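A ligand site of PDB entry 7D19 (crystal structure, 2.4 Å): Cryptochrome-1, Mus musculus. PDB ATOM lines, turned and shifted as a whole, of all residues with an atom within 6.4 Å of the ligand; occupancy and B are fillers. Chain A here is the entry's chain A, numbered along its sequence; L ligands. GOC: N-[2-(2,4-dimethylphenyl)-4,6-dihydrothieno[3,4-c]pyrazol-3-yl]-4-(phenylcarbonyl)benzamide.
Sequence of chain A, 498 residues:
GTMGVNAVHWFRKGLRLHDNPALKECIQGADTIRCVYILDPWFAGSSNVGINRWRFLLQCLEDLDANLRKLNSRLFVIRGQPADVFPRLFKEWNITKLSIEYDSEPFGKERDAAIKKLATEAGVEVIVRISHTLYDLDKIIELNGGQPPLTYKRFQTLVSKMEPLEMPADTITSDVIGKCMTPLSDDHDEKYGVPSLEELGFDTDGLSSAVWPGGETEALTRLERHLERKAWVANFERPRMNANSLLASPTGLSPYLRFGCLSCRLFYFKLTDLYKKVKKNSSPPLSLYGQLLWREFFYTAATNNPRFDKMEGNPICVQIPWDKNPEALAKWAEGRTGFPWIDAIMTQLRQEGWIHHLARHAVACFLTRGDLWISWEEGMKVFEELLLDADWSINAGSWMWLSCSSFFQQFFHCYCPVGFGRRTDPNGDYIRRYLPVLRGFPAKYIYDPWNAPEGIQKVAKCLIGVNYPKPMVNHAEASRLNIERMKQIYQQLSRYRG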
ATOM      1  N   TYR A 152       5.170   7.209  33.512  1.00  0.00           N
ATOM      2  CA  TYR A 152       6.143   6.225  33.962  1.00  0.00           C
ATOM      3  C   TYR A 152       6.857   6.688  35.237  1.00  0.00           C
ATOM      4  O   TYR A 152       7.134   5.869  36.120  1.00  0.00           O
ATOM      5  CB  TYR A 152       7.146   5.977  32.839  1.00  0.00           C
ATOM      6  CG  TYR A 152       8.225   4.955  33.123  1.00  0.00           C
ATOM      7  CD1 TYR A 152       7.897   3.637  33.426  1.00  0.00           C
ATOM      8  CD2 TYR A 152       9.558   5.313  33.076  1.00  0.00           C
ATOM      9  CE1 TYR A 152       8.871   2.700  33.671  1.00  0.00           C
ATOM     10  CE2 TYR A 152      10.545   4.375  33.310  1.00  0.00           C
ATOM     11  CZ  TYR A 152      10.193   3.070  33.620  1.00  0.00           C
ATOM     12  OH  TYR A 152      11.187   2.141  33.862  1.00  0.00           O
ATOM     13  N   SER A 254      13.441 -11.824  25.751  1.00  0.00           N
ATOM     14  CA  SER A 254      12.137 -11.167  25.740  1.00  0.00           C
ATOM     15  C   SER A 254      10.972 -12.064  25.285  1.00  0.00           C
ATOM     16  O   SER A 254       9.929 -12.030  25.948  1.00  0.00           O
ATOM     17  CB  SER A 254      12.191  -9.880  24.907  1.00  0.00           C
ATOM     18  OG  SER A 254      12.282 -10.108  23.518  1.00  0.00           O
ATOM     19  N   GLN A 291      13.861  -3.364  30.258  1.00  0.00           N
ATOM     20  CA  GLN A 291      12.471  -3.199  29.872  1.00  0.00           C
ATOM     21  C   GLN A 291      11.479  -3.665  30.934  1.00  0.00           C
ATOM     22  O   GLN A 291      10.268  -3.520  30.722  1.00  0.00           O
ATOM     23  CB  GLN A 291      12.211  -3.947  28.583  1.00  0.00           C
ATOM     24  CG  GLN A 291      12.634  -5.423  28.731  1.00  0.00           C
ATOM     25  CD  GLN A 291      12.205  -6.322  27.581  1.00  0.00           C
ATOM     26  OE1 GLN A 291      12.393  -5.998  26.400  1.00  0.00           O
ATOM     27  NE2 GLN A 291      11.616  -7.456  27.925  1.00  0.00           N
ATOM     28  N   LEU A 292      11.952  -4.144  32.078  1.00  0.00           N
ATOM     29  CA  LEU A 292      11.088  -4.837  33.034  1.00  0.00           C
ATOM     30  C   LEU A 292      10.025  -3.921  33.608  1.00  0.00           C
ATOM     31  O   LEU A 292       8.887  -4.340  33.787  1.00  0.00           O
ATOM     32  CB  LEU A 292      11.922  -5.437  34.162  1.00  0.00           C
ATOM     33  CG  LEU A 292      12.520  -6.810  33.870  1.00  0.00           C
ATOM     34  CD1 LEU A 292      13.260  -7.392  35.074  1.00  0.00           C
ATOM     35  CD2 LEU A 292      11.423  -7.758  33.373  1.00  0.00           C
ATOM     36  N   TRP A 294       8.946  -0.926  32.310  1.00  0.00           N
ATOM     37  CA  TRP A 294       8.054  -0.479  31.247  1.00  0.00           C
ATOM     38  C   TRP A 294       6.996  -1.535  30.952  1.00  0.00           C
ATOM     39  O   TRP A 294       5.838  -1.202  30.676  1.00  0.00           O
ATOM     40  CB  TRP A 294       8.854  -0.165  29.980  1.00  0.00           C
ATOM     41  CG  TRP A 294       9.405   1.213  29.969  1.00  0.00           C
ATOM     42  CD1 TRP A 294      10.708   1.586  30.171  1.00  0.00           C
ATOM     43  CD2 TRP A 294       8.671   2.433  29.783  1.00  0.00           C
ATOM     44  NE1 TRP A 294      10.828   2.946  30.110  1.00  0.00           N
ATOM     45  CE2 TRP A 294       9.595   3.492  29.860  1.00  0.00           C
ATOM     46  CE3 TRP A 294       7.328   2.724  29.525  1.00  0.00           C
ATOM     47  CZ2 TRP A 294       9.223   4.828  29.699  1.00  0.00           C
ATOM     48  CZ3 TRP A 294       6.960   4.057  29.351  1.00  0.00           C
ATOM     49  CH2 TRP A 294       7.904   5.085  29.444  1.00  0.00           C
ATOM     50  N   ARG A 295       7.401  -2.803  30.979  1.00  0.00           N
ATOM     51  CA  ARG A 295       6.459  -3.911  30.875  1.00  0.00           C
ATOM     52  C   ARG A 295       5.380  -3.806  31.954  1.00  0.00           C
ATOM     53  O   ARG A 295       4.174  -3.790  31.658  1.00  0.00           O
ATOM     54  CB  ARG A 295       7.246  -5.213  30.968  1.00  0.00           C
ATOM     55  CG  ARG A 295       6.497  -6.520  30.904  1.00  0.00           C
ATOM     56  CD  ARG A 295       7.517  -7.667  31.021  1.00  0.00           C
ATOM     57  NE  ARG A 295       6.888  -8.968  30.928  1.00  0.00           N
ATOM     58  CZ  ARG A 295       6.434  -9.646  31.980  1.00  0.00           C
ATOM     59  NH1 ARG A 295       6.554  -9.131  33.199  1.00  0.00           N
ATOM     60  NH2 ARG A 295       5.862 -10.833  31.804  1.00  0.00           N
ATOM     61  N   PHE A 298       2.883  -0.696  31.367  1.00  0.00           N
ATOM     62  CA  PHE A 298       1.813  -0.850  30.378  1.00  0.00           C
ATOM     63  C   PHE A 298       0.763  -1.841  30.841  1.00  0.00           C
ATOM     64  O   PHE A 298      -0.430  -1.647  30.569  1.00  0.00           O
ATOM     65  CB  PHE A 298       2.416  -1.271  29.029  1.00  0.00           C
ATOM     66  CG  PHE A 298       3.174  -0.150  28.333  1.00  0.00           C
ATOM     67  CD1 PHE A 298       2.614   1.125  28.214  1.00  0.00           C
ATOM     68  CD2 PHE A 298       4.442  -0.368  27.826  1.00  0.00           C
ATOM     69  CE1 PHE A 298       3.306   2.157  27.579  1.00  0.00           C
ATOM     70  CE2 PHE A 298       5.143   0.659  27.202  1.00  0.00           C
ATOM     71  CZ  PHE A 298       4.566   1.924  27.072  1.00  0.00           C
ATOM     72  N   HIS A 357      14.764  -2.998  20.012  1.00  0.00           N
ATOM     73  CA  HIS A 357      13.893  -1.950  20.537  1.00  0.00           C
ATOM     74  C   HIS A 357      14.066  -0.629  19.796  1.00  0.00           C
ATOM     75  O   HIS A 357      13.077   0.053  19.493  1.00  0.00           O
ATOM     76  CB  HIS A 357      14.154  -1.758  22.035  1.00  0.00           C
ATOM     77  CG  HIS A 357      13.168  -2.477  22.905  1.00  0.00           C
ATOM     78  ND1 HIS A 357      13.053  -3.846  22.908  1.00  0.00           N
ATOM     79  CD2 HIS A 357      12.248  -2.010  23.776  1.00  0.00           C
ATOM     80  CE1 HIS A 357      12.100  -4.206  23.752  1.00  0.00           C
ATOM     81  NE2 HIS A 357      11.593  -3.109  24.289  1.00  0.00           N
ATOM     82  N   LEU A 358      15.300  -0.262  19.465  1.00  0.00           N
ATOM     83  CA  LEU A 358      15.506   0.974  18.715  1.00  0.00           C
ATOM     84  C   LEU A 358      14.945   0.875  17.296  1.00  0.00           C
ATOM     85  O   LEU A 358      14.472   1.880  16.743  1.00  0.00           O
ATOM     86  CB  LEU A 358      17.001   1.327  18.688  1.00  0.00           C
ATOM     87  CG  LEU A 358      17.516   2.244  19.814  1.00  0.00           C
ATOM     88  CD1 LEU A 358      16.961   1.838  21.185  1.00  0.00           C
ATOM     89  CD2 LEU A 358      19.039   2.277  19.838  1.00  0.00           C
ATOM     90  N   ARG A 360      12.229  -0.810  16.604  1.00  0.00           N
ATOM     91  CA  ARG A 360      10.801  -0.640  16.811  1.00  0.00           C
ATOM     92  C   ARG A 360      10.436   0.850  16.845  1.00  0.00           C
ATOM     93  O   ARG A 360       9.425   1.261  16.257  1.00  0.00           O
ATOM     94  CB  ARG A 360      10.361  -1.327  18.111  1.00  0.00           C
ATOM     95  CG  ARG A 360      10.696  -2.806  18.157  1.00  0.00           C
ATOM     96  CD  ARG A 360      10.392  -3.463  19.524  1.00  0.00           C
ATOM     97  NE  ARG A 360      11.159  -4.708  19.670  1.00  0.00           N
ATOM     98  CZ  ARG A 360      10.814  -5.728  20.451  1.00  0.00           C
ATOM     99  NH1 ARG A 360       9.691  -5.676  21.180  1.00  0.00           N
ATOM    100  NH2 ARG A 360      11.600  -6.805  20.513  1.00  0.00           N
ATOM    101  N   HIS A 361      11.230   1.654  17.557  1.00  0.00           N
ATOM    102  CA  HIS A 361      11.076   3.106  17.554  1.00  0.00           C
ATOM    103  C   HIS A 361      11.119   3.656  16.120  1.00  0.00           C
ATOM    104  O   HIS A 361      10.291   4.500  15.748  1.00  0.00           O
ATOM    105  CB  HIS A 361      12.182   3.769  18.379  1.00  0.00           C
ATOM    106  CG  HIS A 361      11.985   3.666  19.867  1.00  0.00           C
ATOM    107  ND1 HIS A 361      12.139   2.482  20.555  1.00  0.00           N
ATOM    108  CD2 HIS A 361      11.704   4.610  20.800  1.00  0.00           C
ATOM    109  CE1 HIS A 361      11.938   2.693  21.851  1.00  0.00           C
ATOM    110  NE2 HIS A 361      11.671   3.976  22.019  1.00  0.00           N
ATOM    111  N   VAL A 363      10.582   2.206  13.067  1.00  0.00           N
ATOM    112  CA  VAL A 363       9.506   1.929  12.122  1.00  0.00           C
ATOM    113  C   VAL A 363       8.167   2.431  12.646  1.00  0.00           C
ATOM    114  O   VAL A 363       7.250   2.667  11.848  1.00  0.00           O
ATOM    115  CB  VAL A 363       9.433   0.433  11.757  1.00  0.00           C
ATOM    116  CG1 VAL A 363      10.753  -0.025  11.163  1.00  0.00           C
ATOM    117  CG2 VAL A 363       9.011  -0.441  12.954  1.00  0.00           C
ATOM    118  N   ALA A 364       8.045   2.644  13.955  1.00  0.00           N
ATOM    119  CA  ALA A 364       6.831   3.210  14.531  1.00  0.00           C
ATOM    120  C   ALA A 364       6.713   4.703  14.222  1.00  0.00           C
ATOM    121  O   ALA A 364       5.659   5.170  13.785  1.00  0.00           O
ATOM    122  CB  ALA A 364       6.801   2.975  16.043  1.00  0.00           C
ATOM    123  N   PHE A 383       2.156  -5.500  14.448  1.00  0.00           N
ATOM    124  CA  PHE A 383       3.056  -6.017  15.471  1.00  0.00           C
ATOM    125  C   PHE A 383       2.404  -7.158  16.256  1.00  0.00           C
ATOM    126  O   PHE A 383       3.081  -8.136  16.593  1.00  0.00           O
ATOM    127  CB  PHE A 383       3.503  -4.896  16.426  1.00  0.00           C
ATOM    128  CG  PHE A 383       4.750  -4.173  15.976  1.00  0.00           C
ATOM    129  CD1 PHE A 383       5.003  -3.964  14.627  1.00  0.00           C
ATOM    130  CD2 PHE A 383       5.673  -3.692  16.889  1.00  0.00           C
ATOM    131  CE1 PHE A 383       6.146  -3.295  14.210  1.00  0.00           C
ATOM    132  CE2 PHE A 383       6.825  -3.022  16.474  1.00  0.00           C
ATOM    133  CZ  PHE A 383       7.058  -2.821  15.129  1.00  0.00           C
ATOM    134  N   LEU A 387       5.130  -9.917  16.169  1.00  0.00           N
ATOM    135  CA  LEU A 387       6.132  -9.718  17.208  1.00  0.00           C
ATOM    136  C   LEU A 387       5.967 -10.715  18.348  1.00  0.00           C
ATOM    137  O   LEU A 387       4.911 -10.766  18.983  1.00  0.00           O
ATOM    138  CB  LEU A 387       6.014  -8.302  17.764  1.00  0.00           C
ATOM    139  CG  LEU A 387       7.110  -7.792  18.674  1.00  0.00           C
ATOM    140  CD1 LEU A 387       8.459  -7.883  17.972  1.00  0.00           C
ATOM    141  CD2 LEU A 387       6.757  -6.376  19.045  1.00  0.00           C
ATOM    142  N   ASP A 389       7.435 -10.857  21.394  1.00  0.00           N
ATOM    143  CA  ASP A 389       7.700 -10.515  22.792  1.00  0.00           C
ATOM    144  C   ASP A 389       6.816  -9.414  23.342  1.00  0.00           C
ATOM    145  O   ASP A 389       7.101  -8.897  24.434  1.00  0.00           O
ATOM    146  CB  ASP A 389       9.170 -10.136  22.983  1.00  0.00           C
ATOM    147  CG  ASP A 389       9.561  -8.838  22.294  1.00  0.00           C
ATOM    148  OD1 ASP A 389       8.699  -8.159  21.679  1.00  0.00           O
ATOM    149  OD2 ASP A 389      10.759  -8.506  22.349  1.00  0.00           O
ATOM    150  N   ALA A 390       5.751  -9.031  22.649  1.00  0.00           N
ATOM    151  CA  ALA A 390       4.904  -7.950  23.101  1.00  0.00           C
ATOM    152  C   ALA A 390       3.459  -8.409  22.978  1.00  0.00           C
ATOM    153  O   ALA A 390       3.021  -8.781  21.886  1.00  0.00           O
ATOM    154  CB  ALA A 390       5.147  -6.668  22.303  1.00  0.00           C
ATOM    155  N   ILE A 394       1.288  -4.184  26.246  1.00  0.00           N
ATOM    156  CA  ILE A 394       2.557  -3.506  25.992  1.00  0.00           C
ATOM    157  C   ILE A 394       2.615  -2.990  24.559  1.00  0.00           C
ATOM    158  O   ILE A 394       3.218  -1.944  24.290  1.00  0.00           O
ATOM    159  CB  ILE A 394       3.711  -4.458  26.315  1.00  0.00           C
ATOM    160  CG1 ILE A 394       3.637  -4.840  27.784  1.00  0.00           C
ATOM    161  CG2 ILE A 394       5.064  -3.827  25.949  1.00  0.00           C
ATOM    162  CD1 ILE A 394       4.400  -6.076  28.075  1.00  0.00           C
ATOM    163  N   ASN A 395       1.971  -3.705  23.646  1.00  0.00           N
ATOM    164  CA  ASN A 395       1.951  -3.305  22.253  1.00  0.00           C
ATOM    165  C   ASN A 395       1.068  -2.088  22.044  1.00  0.00           C
ATOM    166  O   ASN A 395       1.463  -1.142  21.353  1.00  0.00           O
ATOM    167  CB  ASN A 395       1.463  -4.482  21.413  1.00  0.00           C
ATOM    168  CG  ASN A 395       1.946  -4.433  20.013  1.00  0.00           C
ATOM    169  OD1 ASN A 395       1.265  -4.876  19.112  1.00  0.00           O
ATOM    170  ND2 ASN A 395       3.134  -3.869  19.813  1.00  0.00           N
ATOM    171  N   GLY A 397       0.191   0.111  24.367  1.00  0.00           N
ATOM    172  CA  GLY A 397       0.778   1.234  25.078  1.00  0.00           C
ATOM    173  C   GLY A 397       2.015   1.780  24.377  1.00  0.00           C
ATOM    174  O   GLY A 397       2.251   3.002  24.380  1.00  0.00           O
ATOM    175  N   SER A 398       2.818   0.901  23.783  1.00  0.00           N
ATOM    176  CA  SER A 398       4.044   1.374  23.126  1.00  0.00           C
ATOM    177  C   SER A 398       3.710   2.172  21.878  1.00  0.00           C
ATOM    178  O   SER A 398       4.304   3.230  21.642  1.00  0.00           O
ATOM    179  CB  SER A 398       4.957   0.202  22.792  1.00  0.00           C
ATOM    180  OG  SER A 398       5.482  -0.425  23.969  1.00  0.00           O
ATOM    181  N   TRP A 399       2.758   1.693  21.089  1.00  0.00           N
ATOM    182  CA  TRP A 399       2.379   2.398  19.865  1.00  0.00           C
ATOM    183  C   TRP A 399       1.719   3.740  20.174  1.00  0.00           C
ATOM    184  O   TRP A 399       1.915   4.710  19.436  1.00  0.00           O
ATOM    185  CB  TRP A 399       1.460   1.525  19.020  1.00  0.00           C
ATOM    186  CG  TRP A 399       2.219   0.594  18.164  1.00  0.00           C
ATOM    187  CD1 TRP A 399       2.526  -0.707  18.443  1.00  0.00           C
ATOM    188  CD2 TRP A 399       2.789   0.878  16.879  1.00  0.00           C
ATOM    189  NE1 TRP A 399       3.255  -1.245  17.415  1.00  0.00           N
ATOM    190  CE2 TRP A 399       3.428  -0.300  16.439  1.00  0.00           C
ATOM    191  CE3 TRP A 399       2.834   2.032  16.070  1.00  0.00           C
ATOM    192  CZ2 TRP A 399       4.099  -0.369  15.228  1.00  0.00           C
ATOM    193  CZ3 TRP A 399       3.493   1.956  14.865  1.00  0.00           C
ATOM    194  CH2 TRP A 399       4.120   0.759  14.446  1.00  0.00           C
ATOM    195  N   TRP A 401       2.369   5.624  22.954  1.00  0.00           N
ATOM    196  CA  TRP A 401       3.403   6.500  23.489  1.00  0.00           C
ATOM    197  C   TRP A 401       4.352   6.970  22.386  1.00  0.00           C
ATOM    198  O   TRP A 401       4.718   8.153  22.340  1.00  0.00           O
ATOM    199  CB  TRP A 401       4.177   5.775  24.589  1.00  0.00           C
ATOM    200  CG  TRP A 401       3.803   6.141  26.004  1.00  0.00           C
ATOM    201  CD1 TRP A 401       4.598   6.758  26.940  1.00  0.00           C
ATOM    202  CD2 TRP A 401       2.538   5.902  26.656  1.00  0.00           C
ATOM    203  NE1 TRP A 401       3.913   6.921  28.119  1.00  0.00           N
ATOM    204  CE2 TRP A 401       2.646   6.403  27.976  1.00  0.00           C
ATOM    205  CE3 TRP A 401       1.342   5.312  26.253  1.00  0.00           C
ATOM    206  CZ2 TRP A 401       1.599   6.333  28.889  1.00  0.00           C
ATOM    207  CZ3 TRP A 401       0.295   5.242  27.166  1.00  0.00           C
ATOM    208  CH2 TRP A 401       0.438   5.744  28.466  1.00  0.00           C
ATOM    209  N   LEU A 402       4.755   6.064  21.487  1.00  0.00           N
ATOM    210  CA  LEU A 402       5.728   6.433  20.463  1.00  0.00           C
ATOM    211  C   LEU A 402       5.120   7.238  19.321  1.00  0.00           C
ATOM    212  O   LEU A 402       5.865   7.859  18.557  1.00  0.00           O
ATOM    213  CB  LEU A 402       6.416   5.177  19.906  1.00  0.00           C
ATOM    214  CG  LEU A 402       7.313   4.496  20.943  1.00  0.00           C
ATOM    215  CD1 LEU A 402       7.817   3.136  20.471  1.00  0.00           C
ATOM    216  CD2 LEU A 402       8.478   5.393  21.309  1.00  0.00           C
ATOM    217  N   GLN A 409       3.718  12.487  27.247  1.00  0.00           N
ATOM    218  CA  GLN A 409       4.996  12.105  26.655  1.00  0.00           C
ATOM    219  C   GLN A 409       5.037  12.696  25.251  1.00  0.00           C
ATOM    220  O   GLN A 409       4.523  12.101  24.296  1.00  0.00           O
ATOM    221  CB  GLN A 409       5.174  10.586  26.636  1.00  0.00           C
ATOM    222  CG  GLN A 409       6.546  10.131  26.166  1.00  0.00           C
ATOM    223  CD  GLN A 409       7.664  10.749  26.971  1.00  0.00           C
ATOM    224  OE1 GLN A 409       7.824  10.456  28.150  1.00  0.00           O
ATOM    225  NE2 GLN A 409       8.451  11.609  26.333  1.00  0.00           N
ATOM    226  N   PHE A 411       7.476  13.919  22.225  1.00  0.00           N
ATOM    227  CA  PHE A 411       8.833  13.678  21.751  1.00  0.00           C
ATOM    228  C   PHE A 411       9.272  14.851  20.885  1.00  0.00           C
ATOM    229  O   PHE A 411       8.528  15.314  20.020  1.00  0.00           O
ATOM    230  CB  PHE A 411       8.914  12.362  20.988  1.00  0.00           C
ATOM    231  CG  PHE A 411       8.848  11.146  21.874  1.00  0.00           C
ATOM    232  CD1 PHE A 411       9.898  10.838  22.723  1.00  0.00           C
ATOM    233  CD2 PHE A 411       7.735  10.311  21.866  1.00  0.00           C
ATOM    234  CE1 PHE A 411       9.844   9.721  23.547  1.00  0.00           C
ATOM    235  CE2 PHE A 411       7.683   9.201  22.682  1.00  0.00           C
ATOM    236  CZ  PHE A 411       8.731   8.906  23.528  1.00  0.00           C
HETATM  237  C14 GOC L   1      11.885   6.829  26.020  1.00  0.00           C
HETATM  238  C11 GOC L   1       9.452   7.367  27.201  1.00  0.00           C
HETATM  239  C10 GOC L   1       9.514   6.347  26.230  1.00  0.00           C
HETATM  240  C12 GOC L   1      10.576   8.102  27.564  1.00  0.00           C
HETATM  241  C13 GOC L   1      11.809   7.836  26.967  1.00  0.00           C
HETATM  242  C02 GOC L   1       8.764  -0.330  25.452  1.00  0.00           C
HETATM  243  C03 GOC L   1       8.631   1.109  25.581  1.00  0.00           C
HETATM  244  C04 GOC L   1       9.406   1.863  26.442  1.00  0.00           C
HETATM  245  C05 GOC L   1       9.304   3.253  26.512  1.00  0.00           C
HETATM  246  C06 GOC L   1       7.788   1.871  24.753  1.00  0.00           C
HETATM  247  C07 GOC L   1       7.686   3.261  24.823  1.00  0.00           C
HETATM  248  C08 GOC L   1       8.424   4.009  25.712  1.00  0.00           C
HETATM  249  C09 GOC L   1       8.383   5.491  25.785  1.00  0.00           C
HETATM  250  C15 GOC L   1      10.766   6.097  25.672  1.00  0.00           C
HETATM  251  C18 GOC L   1       8.110  -2.459  24.472  1.00  0.00           C
HETATM  252  C19 GOC L   1       8.392  -3.517  25.337  1.00  0.00           C
HETATM  253  C20 GOC L   1       8.644  -3.717  26.776  1.00  0.00           C
HETATM  254  C22 GOC L   1       8.662  -5.990  25.274  1.00  0.00           C
HETATM  255  C23 GOC L   1       8.394  -4.716  24.538  1.00  0.00           C
HETATM  256  C26 GOC L   1       7.667  -2.221  21.984  1.00  0.00           C
HETATM  257  C27 GOC L   1       8.409  -1.079  21.517  1.00  0.00           C
HETATM  258  C28 GOC L   1       9.667  -0.572  22.182  1.00  0.00           C
HETATM  259  C29 GOC L   1       7.991  -0.386  20.380  1.00  0.00           C
HETATM  260  C30 GOC L   1       6.524  -2.535  21.256  1.00  0.00           C
HETATM  261  C31 GOC L   1       6.135  -1.812  20.108  1.00  0.00           C
HETATM  262  C32 GOC L   1       6.870  -0.699  19.642  1.00  0.00           C
HETATM  263  C33 GOC L   1       6.474   0.088  18.402  1.00  0.00           C
HETATM  264  N17 GOC L   1       7.990  -1.133  24.694  1.00  0.00           N
HETATM  265  N24 GOC L   1       8.152  -4.377  23.243  1.00  0.00           N
HETATM  266  N25 GOC L   1       7.990  -2.987  23.217  1.00  0.00           N
HETATM  267  O01 GOC L   1       9.733  -0.877  25.981  1.00  0.00           O
HETATM  268  O16 GOC L   1       7.366   6.030  25.370  1.00  0.00           O
HETATM  269  S21 GOC L   1       8.466  -5.521  27.059  1.00  0.00           S
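CE2 of Trp 294 touches C05 of the ligand, at 3.4 Å. CE2 of Phe 298 touches C06 of the ligand (3.8 Å). His 361 touches the ligand (CE1 to C28, 3.99 Å). CB of Ala 364 touches C33 of the ligand (3.7 Å). CE2 of Phe 383 touches C33 of the ligand, at 3.7 Å. Asp 389 touches the ligand (O to C22, 3.4 Å). Ala 390 touches the ligand. CG2 of Ile 394 touches C19 of the ligand, 3.4 Å away. ND2 of Asn 395 touches C31 of the ligand, at 3.7 Å. Trp 399 touches the ligand. Trp 401 touches the ligand. Leu 402 touches the ligand (CD1 to C29, 3.5 Å). Gln 409 touches the ligand (OE1 to C11, 3.6 Å). Phe 411 touches the ligand (CZ to O16, 3.7 Å). Hydrophobic or aromatic side chains that line the ligand: Trp 294, Phe 298, His 357, His 361, Ala 364, Phe 383, Ala 390, Ile 394, Trp 399, Trp 401, Leu 402 and Phe 411. Of the 26 residues printed, 18 come within 4 Å of the ligand. The nearest printed residue that does not touch the ligand is Arg 295 (4.1 Å).
S21 of the ligand lies close to NE2 of Gln 291, at 3.8 Å. NH1 of Arg 360 is in hydrogen-bond range of N24 of the ligand. NE2 of His 357 sits at hydrogen-bond distance from O01 of the ligand. The side-chain hydroxyl (OG) of Ser 398 sits at hydrogen-bond distance from a nitrogen (N17) of the ligand (2.7 Å).
ND1 of His 361 sits at hydrogen-bond distance from O of His 357, 2.8 Å away. NH2 of Arg 360 lies within salt-bridge range of OD2 of Asp 389. OD2 of Asp 389 sits at hydrogen-bond distance from OG of Ser 254 (2.5 Å). O of Ile 394 is in hydrogen-bond range of OG of Ser 398 (2.7 Å).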
